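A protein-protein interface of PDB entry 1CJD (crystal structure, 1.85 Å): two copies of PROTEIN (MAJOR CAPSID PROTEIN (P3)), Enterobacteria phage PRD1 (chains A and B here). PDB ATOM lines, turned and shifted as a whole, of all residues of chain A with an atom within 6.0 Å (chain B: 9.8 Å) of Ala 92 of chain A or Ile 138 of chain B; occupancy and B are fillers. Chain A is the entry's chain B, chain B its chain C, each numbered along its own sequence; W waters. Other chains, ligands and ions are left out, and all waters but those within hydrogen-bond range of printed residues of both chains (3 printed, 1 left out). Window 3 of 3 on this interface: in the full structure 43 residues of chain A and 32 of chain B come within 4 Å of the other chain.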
ATOM      1  N   LEU A  86       8.524   6.754 -24.744  1.00  0.00           N
ATOM      2  CA  LEU A  86       8.831   8.171 -24.630  1.00  0.00           C
ATOM      3  C   LEU A  86       8.654   8.863 -25.968  1.00  0.00           C
ATOM      4  O   LEU A  86       8.949   8.273 -27.010  1.00  0.00           O
ATOM      5  CB  LEU A  86      10.299   8.366 -24.207  1.00  0.00           C
ATOM      6  CG  LEU A  86      10.676   8.173 -22.744  1.00  0.00           C
ATOM      7  CD1 LEU A  86      12.204   8.328 -22.614  1.00  0.00           C
ATOM      8  CD2 LEU A  86       9.937   9.211 -21.846  1.00  0.00           C
ATOM      9  N   THR A  87       8.183  10.112 -25.935  1.00  0.00           N
ATOM     10  CA  THR A  87       8.089  10.930 -27.142  1.00  0.00           C
ATOM     11  C   THR A  87       9.529  11.478 -27.325  1.00  0.00           C
ATOM     12  O   THR A  87      10.414  11.188 -26.502  1.00  0.00           O
ATOM     13  CB  THR A  87       7.176  12.147 -26.947  1.00  0.00           C
ATOM     14  OG1 THR A  87       7.637  12.891 -25.812  1.00  0.00           O
ATOM     15  CG2 THR A  87       5.703  11.706 -26.730  1.00  0.00           C
ATOM     16  N   ASP A  88       9.761  12.271 -28.368  1.00  0.00           N
ATOM     17  CA  ASP A  88      11.101  12.828 -28.594  1.00  0.00           C
ATOM     18  C   ASP A  88      11.543  13.758 -27.446  1.00  0.00           C
ATOM     19  O   ASP A  88      12.718  13.771 -27.078  1.00  0.00           O
ATOM     20  CB  ASP A  88      11.161  13.615 -29.922  1.00  0.00           C
ATOM     21  CG  ASP A  88      11.114  12.719 -31.161  1.00  0.00           C
ATOM     22  OD1 ASP A  88      11.166  11.480 -31.040  1.00  0.00           O
ATOM     23  OD2 ASP A  88      11.013  13.273 -32.276  1.00  0.00           O
ATOM     24  N   PHE A  89      10.608  14.535 -26.885  1.00  0.00           N
ATOM     25  CA  PHE A  89      10.939  15.461 -25.806  1.00  0.00           C
ATOM     26  C   PHE A  89      10.900  14.768 -24.439  1.00  0.00           C
ATOM     27  O   PHE A  89      11.615  15.163 -23.518  1.00  0.00           O
ATOM     28  CB  PHE A  89       9.999  16.688 -25.823  1.00  0.00           C
ATOM     29  CG  PHE A  89      10.109  17.549 -27.071  1.00  0.00           C
ATOM     30  CD1 PHE A  89      10.915  17.174 -28.147  1.00  0.00           C
ATOM     31  CD2 PHE A  89       9.358  18.730 -27.185  1.00  0.00           C
ATOM     32  CE1 PHE A  89      10.964  17.970 -29.330  1.00  0.00           C
ATOM     33  CE2 PHE A  89       9.403  19.516 -28.343  1.00  0.00           C
ATOM     34  CZ  PHE A  89      10.200  19.141 -29.415  1.00  0.00           C
ATOM     35  N   GLY A  90      10.047  13.749 -24.313  1.00  0.00           N
ATOM     36  CA  GLY A  90       9.948  12.979 -23.082  1.00  0.00           C
ATOM     37  C   GLY A  90       9.859  13.758 -21.783  1.00  0.00           C
ATOM     38  O   GLY A  90       8.976  14.614 -21.614  1.00  0.00           O
ATOM     39  N   PRO A  91      10.797  13.534 -20.848  1.00  0.00           N
ATOM     40  CA  PRO A  91      10.740  14.260 -19.566  1.00  0.00           C
ATOM     41  C   PRO A  91      10.894  15.776 -19.662  1.00  0.00           C
ATOM     42  O   PRO A  91      10.588  16.489 -18.721  1.00  0.00           O
ATOM     43  CB  PRO A  91      11.849  13.614 -18.733  1.00  0.00           C
ATOM     44  CG  PRO A  91      12.817  13.059 -19.777  1.00  0.00           C
ATOM     45  CD  PRO A  91      11.986  12.667 -20.969  1.00  0.00           C
ATOM     46  N   ALA A  92      11.367  16.279 -20.792  1.00  0.00           N
ATOM     47  CA  ALA A  92      11.509  17.719 -20.927  1.00  0.00           C
ATOM     48  C   ALA A  92      10.113  18.340 -20.932  1.00  0.00           C
ATOM     49  O   ALA A  92       9.970  19.559 -20.772  1.00  0.00           O
ATOM     50  CB  ALA A  92      12.252  18.077 -22.205  1.00  0.00           C
ATOM     51  N   ASN A  93       9.085  17.498 -21.106  1.00  0.00           N
ATOM     52  CA  ASN A  93       7.699  17.981 -21.104  1.00  0.00           C
ATOM     53  C   ASN A  93       6.991  17.881 -19.714  1.00  0.00           C
ATOM     54  O   ASN A  93       5.759  18.069 -19.598  1.00  0.00           O
ATOM     55  CB  ASN A  93       6.907  17.257 -22.199  1.00  0.00           C
ATOM     56  CG  ASN A  93       7.025  17.966 -23.563  1.00  0.00           C
ATOM     57  OD1 ASN A  93       7.276  19.191 -23.624  1.00  0.00           O
ATOM     58  ND2 ASN A  93       6.846  17.210 -24.657  1.00  0.00           N
ATOM     59  N   LEU A  94       7.767  17.606 -18.663  1.00  0.00           N
ATOM     60  CA  LEU A  94       7.223  17.527 -17.299  1.00  0.00           C
ATOM     61  C   LEU A  94       6.764  18.928 -16.891  1.00  0.00           C
ATOM     62  O   LEU A  94       5.804  19.077 -16.140  1.00  0.00           O
ATOM     63  CB  LEU A  94       8.268  17.000 -16.305  1.00  0.00           C
ATOM     64  CG  LEU A  94       8.277  15.467 -16.195  1.00  0.00           C
ATOM     65  CD1 LEU A  94       9.542  14.934 -15.468  1.00  0.00           C
ATOM     66  CD2 LEU A  94       7.009  15.048 -15.454  1.00  0.00           C
ATOM     67  N   VAL A  95       7.469  19.954 -17.365  1.00  0.00           N
ATOM     68  CA  VAL A  95       7.035  21.337 -17.108  1.00  0.00           C
ATOM     69  C   VAL A  95       6.522  21.815 -18.471  1.00  0.00           C
ATOM     70  O   VAL A  95       7.247  21.744 -19.470  1.00  0.00           O
ATOM     71  CB  VAL A  95       8.180  22.269 -16.627  1.00  0.00           C
ATOM     72  CG1 VAL A  95       7.778  23.705 -16.777  1.00  0.00           C
ATOM     73  CG2 VAL A  95       8.477  22.002 -15.167  1.00  0.00           C
ATOM     74  N   GLN A  96       5.263  22.251 -18.527  1.00  0.00           N
ATOM     75  CA  GLN A  96       4.682  22.743 -19.773  1.00  0.00           C
ATOM     76  C   GLN A  96       5.055  24.202 -20.043  1.00  0.00           C
ATOM     77  O   GLN A  96       5.461  24.561 -21.155  1.00  0.00           O
ATOM     78  CB  GLN A  96       3.153  22.585 -19.724  1.00  0.00           C
ATOM     79  CG  GLN A  96       2.709  21.128 -19.783  1.00  0.00           C
ATOM     80  CD  GLN A  96       2.907  20.521 -21.169  1.00  0.00           C
ATOM     81  OE1 GLN A  96       2.180  20.864 -22.095  1.00  0.00           O
ATOM     82  NE2 GLN A  96       3.896  19.614 -21.318  1.00  0.00           N
ATOM     83  N   GLY A 113       8.540  24.299 -21.360  1.00  0.00           N
ATOM     84  CA  GLY A 113       9.577  23.494 -20.750  1.00  0.00           C
ATOM     85  C   GLY A 113      10.539  22.953 -21.805  1.00  0.00           C
ATOM     86  O   GLY A 113      11.775  22.981 -21.627  1.00  0.00           O
ATOM     87  N   TRP A 114      10.006  22.453 -22.914  1.00  0.00           N
ATOM     88  CA  TRP A 114      10.903  21.935 -23.924  1.00  0.00           C
ATOM     89  C   TRP A 114      11.838  23.016 -24.472  1.00  0.00           C
ATOM     90  O   TRP A 114      13.017  22.746 -24.692  1.00  0.00           O
ATOM     91  CB  TRP A 114      10.136  21.240 -25.067  1.00  0.00           C
ATOM     92  CG  TRP A 114       9.125  22.070 -25.856  1.00  0.00           C
ATOM     93  CD1 TRP A 114       7.750  22.058 -25.719  1.00  0.00           C
ATOM     94  CD2 TRP A 114       9.410  22.981 -26.928  1.00  0.00           C
ATOM     95  NE1 TRP A 114       7.176  22.908 -26.639  1.00  0.00           N
ATOM     96  CE2 TRP A 114       8.165  23.487 -27.390  1.00  0.00           C
ATOM     97  CE3 TRP A 114      10.595  23.419 -27.545  1.00  0.00           C
ATOM     98  CZ2 TRP A 114       8.079  24.408 -28.432  1.00  0.00           C
ATOM     99  CZ3 TRP A 114      10.513  24.323 -28.574  1.00  0.00           C
ATOM    100  CH2 TRP A 114       9.262  24.817 -29.013  1.00  0.00           C
ATOM    101  N   HIS A 117      14.587  23.815 -21.913  1.00  0.00           N
ATOM    102  CA  HIS A 117      15.525  22.710 -21.877  1.00  0.00           C
ATOM    103  C   HIS A 117      16.502  22.717 -23.061  1.00  0.00           C
ATOM    104  O   HIS A 117      17.692  22.493 -22.864  1.00  0.00           O
ATOM    105  CB  HIS A 117      14.794  21.375 -21.850  1.00  0.00           C
ATOM    106  CG  HIS A 117      15.697  20.213 -22.107  1.00  0.00           C
ATOM    107  ND1 HIS A 117      16.651  19.806 -21.194  1.00  0.00           N
ATOM    108  CD2 HIS A 117      15.838  19.413 -23.193  1.00  0.00           C
ATOM    109  CE1 HIS A 117      17.344  18.802 -21.711  1.00  0.00           C
ATOM    110  NE2 HIS A 117      16.874  18.546 -22.921  1.00  0.00           N
ATOM    111  N   PHE A 118      16.015  22.977 -24.277  1.00  0.00           N
ATOM    112  CA  PHE A 118      16.909  22.999 -25.434  1.00  0.00           C
ATOM    113  C   PHE A 118      17.944  24.110 -25.278  1.00  0.00           C
ATOM    114  O   PHE A 118      19.103  23.947 -25.698  1.00  0.00           O
ATOM    115  CB  PHE A 118      16.127  23.182 -26.734  1.00  0.00           C
ATOM    116  CG  PHE A 118      15.346  21.961 -27.127  1.00  0.00           C
ATOM    117  CD1 PHE A 118      15.772  20.687 -26.726  1.00  0.00           C
ATOM    118  CD2 PHE A 118      14.155  22.070 -27.845  1.00  0.00           C
ATOM    119  CE1 PHE A 118      15.015  19.531 -27.028  1.00  0.00           C
ATOM    120  CE2 PHE A 118      13.399  20.924 -28.152  1.00  0.00           C
ATOM    121  CZ  PHE A 118      13.830  19.662 -27.741  1.00  0.00           C
ATOM    122  N   ILE A 147      18.980  13.242 -14.975  1.00  0.00           N
ATOM    123  CA  ILE A 147      17.856  13.482 -15.879  1.00  0.00           C
ATOM    124  C   ILE A 147      17.630  12.082 -16.419  1.00  0.00           C
ATOM    125  O   ILE A 147      18.510  11.490 -17.089  1.00  0.00           O
ATOM    126  CB  ILE A 147      18.161  14.471 -16.975  1.00  0.00           C
ATOM    127  CG1 ILE A 147      18.219  15.879 -16.350  1.00  0.00           C
ATOM    128  CG2 ILE A 147      17.038  14.401 -18.072  1.00  0.00           C
ATOM    129  CD1 ILE A 147      18.369  17.034 -17.364  1.00  0.00           C
ATOM    130  N   MET A 163      13.807  15.174 -13.912  1.00  0.00           N
ATOM    131  CA  MET A 163      14.118  16.201 -14.888  1.00  0.00           C
ATOM    132  C   MET A 163      14.623  17.465 -14.182  1.00  0.00           C
ATOM    133  O   MET A 163      14.195  17.770 -13.078  1.00  0.00           O
ATOM    134  CB  MET A 163      12.855  16.528 -15.701  1.00  0.00           C
ATOM    135  CG  MET A 163      13.043  17.579 -16.795  1.00  0.00           C
ATOM    136  SD  MET A 163      14.221  17.018 -18.051  1.00  0.00           S
ATOM    137  CE  MET A 163      14.571  18.574 -18.911  1.00  0.00           C
ATOM    138  N   TYR A 165      15.591  21.728 -14.816  1.00  0.00           N
ATOM    139  CA  TYR A 165      15.545  22.890 -15.689  1.00  0.00           C
ATOM    140  C   TYR A 165      16.293  24.019 -14.970  1.00  0.00           C
ATOM    141  O   TYR A 165      16.176  24.169 -13.749  1.00  0.00           O
ATOM    142  CB  TYR A 165      14.105  23.393 -15.933  1.00  0.00           C
ATOM    143  CG  TYR A 165      13.124  22.412 -16.555  1.00  0.00           C
ATOM    144  CD1 TYR A 165      12.333  21.580 -15.746  1.00  0.00           C
ATOM    145  CD2 TYR A 165      12.957  22.349 -17.955  1.00  0.00           C
ATOM    146  CE1 TYR A 165      11.391  20.709 -16.315  1.00  0.00           C
ATOM    147  CE2 TYR A 165      12.012  21.477 -18.541  1.00  0.00           C
ATOM    148  CZ  TYR A 165      11.236  20.670 -17.709  1.00  0.00           C
ATOM    149  OH  TYR A 165      10.306  19.840 -18.267  1.00  0.00           O
ATOM    150  N   PRO A 336      16.512  16.804 -31.170  1.00  0.00           N
ATOM    151  CA  PRO A 336      15.543  15.819 -31.688  1.00  0.00           C
ATOM    152  C   PRO A 336      14.952  16.126 -33.085  1.00  0.00           C
ATOM    153  O   PRO A 336      15.073  17.236 -33.621  1.00  0.00           O
ATOM    154  CB  PRO A 336      14.460  15.757 -30.593  1.00  0.00           C
ATOM    155  CG  PRO A 336      15.157  16.248 -29.332  1.00  0.00           C
ATOM    156  CD  PRO A 336      16.115  17.315 -29.839  1.00  0.00           C
ATOM    157  N   MET B 132      28.011  12.556 -30.028  1.00  0.00           N
ATOM    158  CA  MET B 132      28.450  11.953 -28.769  1.00  0.00           C
ATOM    159  C   MET B 132      27.292  11.143 -28.175  1.00  0.00           C
ATOM    160  O   MET B 132      26.152  11.584 -28.241  1.00  0.00           O
ATOM    161  CB  MET B 132      28.826  13.105 -27.827  1.00  0.00           C
ATOM    162  CG  MET B 132      29.470  12.730 -26.514  1.00  0.00           C
ATOM    163  SD  MET B 132      29.429  14.149 -25.322  1.00  0.00           S
ATOM    164  CE  MET B 132      28.010  14.963 -25.804  1.00  0.00           C
ATOM    165  N   VAL B 133      27.561   9.980 -27.597  1.00  0.00           N
ATOM    166  CA  VAL B 133      26.494   9.165 -27.007  1.00  0.00           C
ATOM    167  C   VAL B 133      26.373   9.535 -25.519  1.00  0.00           C
ATOM    168  O   VAL B 133      27.401   9.647 -24.830  1.00  0.00           O
ATOM    169  CB  VAL B 133      26.821   7.652 -27.118  1.00  0.00           C
ATOM    170  CG1 VAL B 133      25.811   6.850 -26.321  1.00  0.00           C
ATOM    171  CG2 VAL B 133      26.875   7.221 -28.603  1.00  0.00           C
ATOM    172  N   THR B 134      25.152   9.756 -25.022  1.00  0.00           N
ATOM    173  CA  THR B 134      24.962  10.097 -23.609  1.00  0.00           C
ATOM    174  C   THR B 134      23.753   9.334 -23.071  1.00  0.00           C
ATOM    175  O   THR B 134      23.045   8.694 -23.850  1.00  0.00           O
ATOM    176  CB  THR B 134      24.705  11.627 -23.379  1.00  0.00           C
ATOM    177  OG1 THR B 134      23.314  11.932 -23.588  1.00  0.00           O
ATOM    178  CG2 THR B 134      25.559  12.497 -24.309  1.00  0.00           C
ATOM    179  N   ASP B 135      23.517   9.409 -21.756  1.00  0.00           N
ATOM    180  CA  ASP B 135      22.373   8.742 -21.119  1.00  0.00           C
ATOM    181  C   ASP B 135      21.085   9.595 -21.213  1.00  0.00           C
ATOM    182  O   ASP B 135      20.057   9.232 -20.626  1.00  0.00           O
ATOM    183  CB  ASP B 135      22.647   8.494 -19.628  1.00  0.00           C
ATOM    184  CG  ASP B 135      22.596   9.788 -18.799  1.00  0.00           C
ATOM    185  OD1 ASP B 135      22.746  10.885 -19.378  1.00  0.00           O
ATOM    186  OD2 ASP B 135      22.419   9.734 -17.555  1.00  0.00           O
ATOM    187  N   SER B 136      21.112  10.715 -21.926  1.00  0.00           N
ATOM    188  CA  SER B 136      19.914  11.558 -21.956  1.00  0.00           C
ATOM    189  C   SER B 136      18.663  10.858 -22.491  1.00  0.00           C
ATOM    190  O   SER B 136      18.723  10.246 -23.566  1.00  0.00           O
ATOM    191  CB  SER B 136      20.167  12.801 -22.802  1.00  0.00           C
ATOM    192  OG  SER B 136      19.145  13.768 -22.567  1.00  0.00           O
ATOM    193  N   PRO B 137      17.530  10.891 -21.727  1.00  0.00           N
ATOM    194  CA  PRO B 137      16.254  10.266 -22.174  1.00  0.00           C
ATOM    195  C   PRO B 137      15.591  11.102 -23.308  1.00  0.00           C
ATOM    196  O   PRO B 137      14.787  10.593 -24.098  1.00  0.00           O
ATOM    197  CB  PRO B 137      15.400  10.217 -20.910  1.00  0.00           C
ATOM    198  CG  PRO B 137      15.971  11.315 -20.008  1.00  0.00           C
ATOM    199  CD  PRO B 137      17.442  11.434 -20.352  1.00  0.00           C
ATOM    200  N   ILE B 138      15.947  12.385 -23.380  1.00  0.00           N
ATOM    201  CA  ILE B 138      15.452  13.277 -24.422  1.00  0.00           C
ATOM    202  C   ILE B 138      16.134  12.725 -25.686  1.00  0.00           C
ATOM    203  O   ILE B 138      17.325  12.352 -25.655  1.00  0.00           O
ATOM    204  CB  ILE B 138      15.860  14.760 -24.135  1.00  0.00           C
ATOM    205  CG1 ILE B 138      15.030  15.310 -22.949  1.00  0.00           C
ATOM    206  CG2 ILE B 138      15.559  15.642 -25.347  1.00  0.00           C
ATOM    207  CD1 ILE B 138      15.715  15.279 -21.569  1.00  0.00           C
ATOM    208  N   LYS B 139      15.404  12.668 -26.801  1.00  0.00           N
ATOM    209  CA  LYS B 139      15.956  12.052 -28.004  1.00  0.00           C
ATOM    210  C   LYS B 139      16.950  12.788 -28.920  1.00  0.00           C
ATOM    211  O   LYS B 139      16.722  12.948 -30.136  1.00  0.00           O
ATOM    212  CB  LYS B 139      14.808  11.417 -28.812  1.00  0.00           C
ATOM    213  CG  LYS B 139      13.975  10.456 -27.923  1.00  0.00           C
ATOM    214  CD  LYS B 139      13.311   9.322 -28.676  1.00  0.00           C
ATOM    215  CE  LYS B 139      12.596   8.417 -27.690  1.00  0.00           C
ATOM    216  NZ  LYS B 139      11.565   7.528 -28.312  1.00  0.00           N
ATOM    217  N   TYR B 140      18.056  13.216 -28.292  1.00  0.00           N
ATOM    218  CA  TYR B 140      19.215  13.815 -28.974  1.00  0.00           C
ATOM    219  C   TYR B 140      19.888  12.541 -29.513  1.00  0.00           C
ATOM    220  O   TYR B 140      19.541  11.443 -29.078  1.00  0.00           O
ATOM    221  CB  TYR B 140      20.211  14.416 -27.967  1.00  0.00           C
ATOM    222  CG  TYR B 140      19.692  15.583 -27.198  1.00  0.00           C
ATOM    223  CD1 TYR B 140      19.701  16.850 -27.758  1.00  0.00           C
ATOM    224  CD2 TYR B 140      19.199  15.435 -25.909  1.00  0.00           C
ATOM    225  CE1 TYR B 140      19.231  17.958 -27.056  1.00  0.00           C
ATOM    226  CE2 TYR B 140      18.722  16.545 -25.196  1.00  0.00           C
ATOM    227  CZ  TYR B 140      18.749  17.805 -25.790  1.00  0.00           C
ATOM    228  OH  TYR B 140      18.330  18.933 -25.117  1.00  0.00           O
ATOM    229  N   GLY B 141      20.862  12.670 -30.406  1.00  0.00           N
ATOM    230  CA  GLY B 141      21.532  11.484 -30.893  1.00  0.00           C
ATOM    231  C   GLY B 141      21.855  11.649 -32.350  1.00  0.00           C
ATOM    232  O   GLY B 141      21.910  12.779 -32.850  1.00  0.00           O
ATOM    233  N   ASP B 142      22.093  10.531 -33.032  1.00  0.00           N
ATOM    234  CA  ASP B 142      22.377  10.576 -34.461  1.00  0.00           C
ATOM    235  C   ASP B 142      20.993  10.693 -35.098  1.00  0.00           C
ATOM    236  O   ASP B 142      20.373   9.702 -35.436  1.00  0.00           O
ATOM    237  CB  ASP B 142      23.080   9.282 -34.897  1.00  0.00           C
ATOM    238  CG  ASP B 142      23.343   9.228 -36.388  1.00  0.00           C
ATOM    239  OD1 ASP B 142      23.062  10.251 -37.056  1.00  0.00           O
ATOM    240  OD2 ASP B 142      23.830   8.165 -36.881  1.00  0.00           O
ATOM    241  N   VAL B 143      20.514  11.917 -35.243  1.00  0.00           N
ATOM    242  CA  VAL B 143      19.185  12.160 -35.789  1.00  0.00           C
ATOM    243  C   VAL B 143      19.277  12.478 -37.262  1.00  0.00           C
ATOM    244  O   VAL B 143      18.480  11.987 -38.073  1.00  0.00           O
ATOM    245  CB  VAL B 143      18.487  13.417 -35.082  1.00  0.00           C
ATOM    246  CG1 VAL B 143      17.174  13.808 -35.800  1.00  0.00           C
ATOM    247  CG2 VAL B 143      18.245  13.136 -33.625  1.00  0.00           C
HETATM  248  O   HOH W   1      20.646  12.487 -18.672  1.00  0.00           O
HETATM  249  O   HOH W   2      20.204   9.687 -16.367  1.00  0.00           O
HETATM  250  O   HOH W   3       9.887   9.152 -30.176  1.00  0.00           O
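N of Gly 90 of chain A sits at hydrogen-bond distance from OG1 of Thr 87 of chain A (3.0 Å). The side-chain hydroxyl of Tyr 165 of chain A is in hydrogen-bond range of the backbone carbonyl oxygen of Pro 91 of chain A, 3.4 Å away. The backbone carbonyl oxygen of Ala 92 of chain A lies within hydrogen-bond range of the side-chain hydroxyl of Tyr 165 of chain A (2.5 Å).
Printed residues of chain B that touch a printed residue of chain A: Pro 137, Ile 138, Lys 139 and Tyr 140. Printed residues of chain A that touch a printed residue of chain B: Leu 86, Thr 87, Asp 88, Phe 89, Pro 91, Ala 92, His 117, Phe 118, Ile 147 and Pro 336. Among the printed residues, 14 pairs touch across the chains.
The side-chain amino group of Lys 139 of chain B lies within hydrogen-bond range of the backbone carbonyl oxygen of Leu 86 of chain A (3.0 Å). O of Asp 88 of chain A lies within hydrogen-bond range of N of Lys 139 of chain B, 2.9 Å away. A ring nitrogen (NE2) of His 117 of chain A is in hydrogen-bond range of the side-chain hydroxyl (OH) of Tyr 140 of chain B.
Pro 137 of chain B touches Leu 86 of chain A. Thr 87 of chain A touches Lys 139 of chain B. O of Asp 88 of chain A touches CG2 of Ile 138 of chain B, 3.8 Å away. O of Phe 89 of chain A touches CG1 of Ile 138 of chain B, at 3.5 Å. CG1 of Ile 138 of chain B touches CB of Ala 92 of chain A (3.99 Å). His 117 of chain A touches Ile 138 of chain B. OH of Tyr 140 of chain B touches CD1 of Phe 118 of chain A, 3.5 Å away. Pro 137 of chain B touches Ile 147 of chain A. Ile 138 of chain B touches Ile 147 of chain A (CD1 to CG2, 3.8 Å). O of Lys 139 of chain B touches CA of Pro 336 of chain A, 3.5 Å away.
Printed residues of chain B within 4 Å of Ala 92 of chain A: Ile 138. Printed residues of chain A within 4 Å of Ile 138 of chain B: Asp 88 (3.8 Å), Phe 89 (3.5 Å), Ala 92 (3.99 Å), His 117 (3.7 Å) and Ile 147 (3.8 Å). No residue of chain B comes within 4 Å of Gly 90 of chain A. Printed residues of chain B within 4 Å of Phe 89 of chain A: Ile 138 (3.5 Å). Of the printed residues of chain B, His 117 of chain A touches Ile 138 and Tyr 140. Printed residues of chain B within 4 Å of Thr 87 of chain A: Lys 139. Of the printed residues of chain B, Phe 118 of chain A touches Tyr 140. The nearest printed residue of chain B that does not touch Ala 92 of chain A is Tyr 140 of chain B (6.8 Å). The nearest printed residue of chain A that does not touch Ile 138 of chain B is Pro 336 of chain A (4.1 Å). The nearest printed residue of chain A that does not touch Pro 137 of chain B is Asp 88 of chain A (4.8 Å).
No position is printed for both chains. Of the 14 pairs that touch across the chains among the printed residues, none has its exchanged pair printed and touching as well.
Water W2 bridges the side-chain carboxylate (OD2) of Asp 135 of chain B (2.5 Å) and the backbone carbonyl oxygen (O) of Ile 147 of chain A (2.6 Å). Water W1 bridges OD1 of Asp 135 of chain B and O of Ile 147 of chain A. Water W3 lies within hydrogen-bond range of the side-chain carboxylate of Asp 88 of chain A (2.8 Å), the side-chain amino group of Lys 139 of chain B (3.0 Å) and the backbone carbonyl oxygen of Leu 86 of chain A (3.4 Å).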
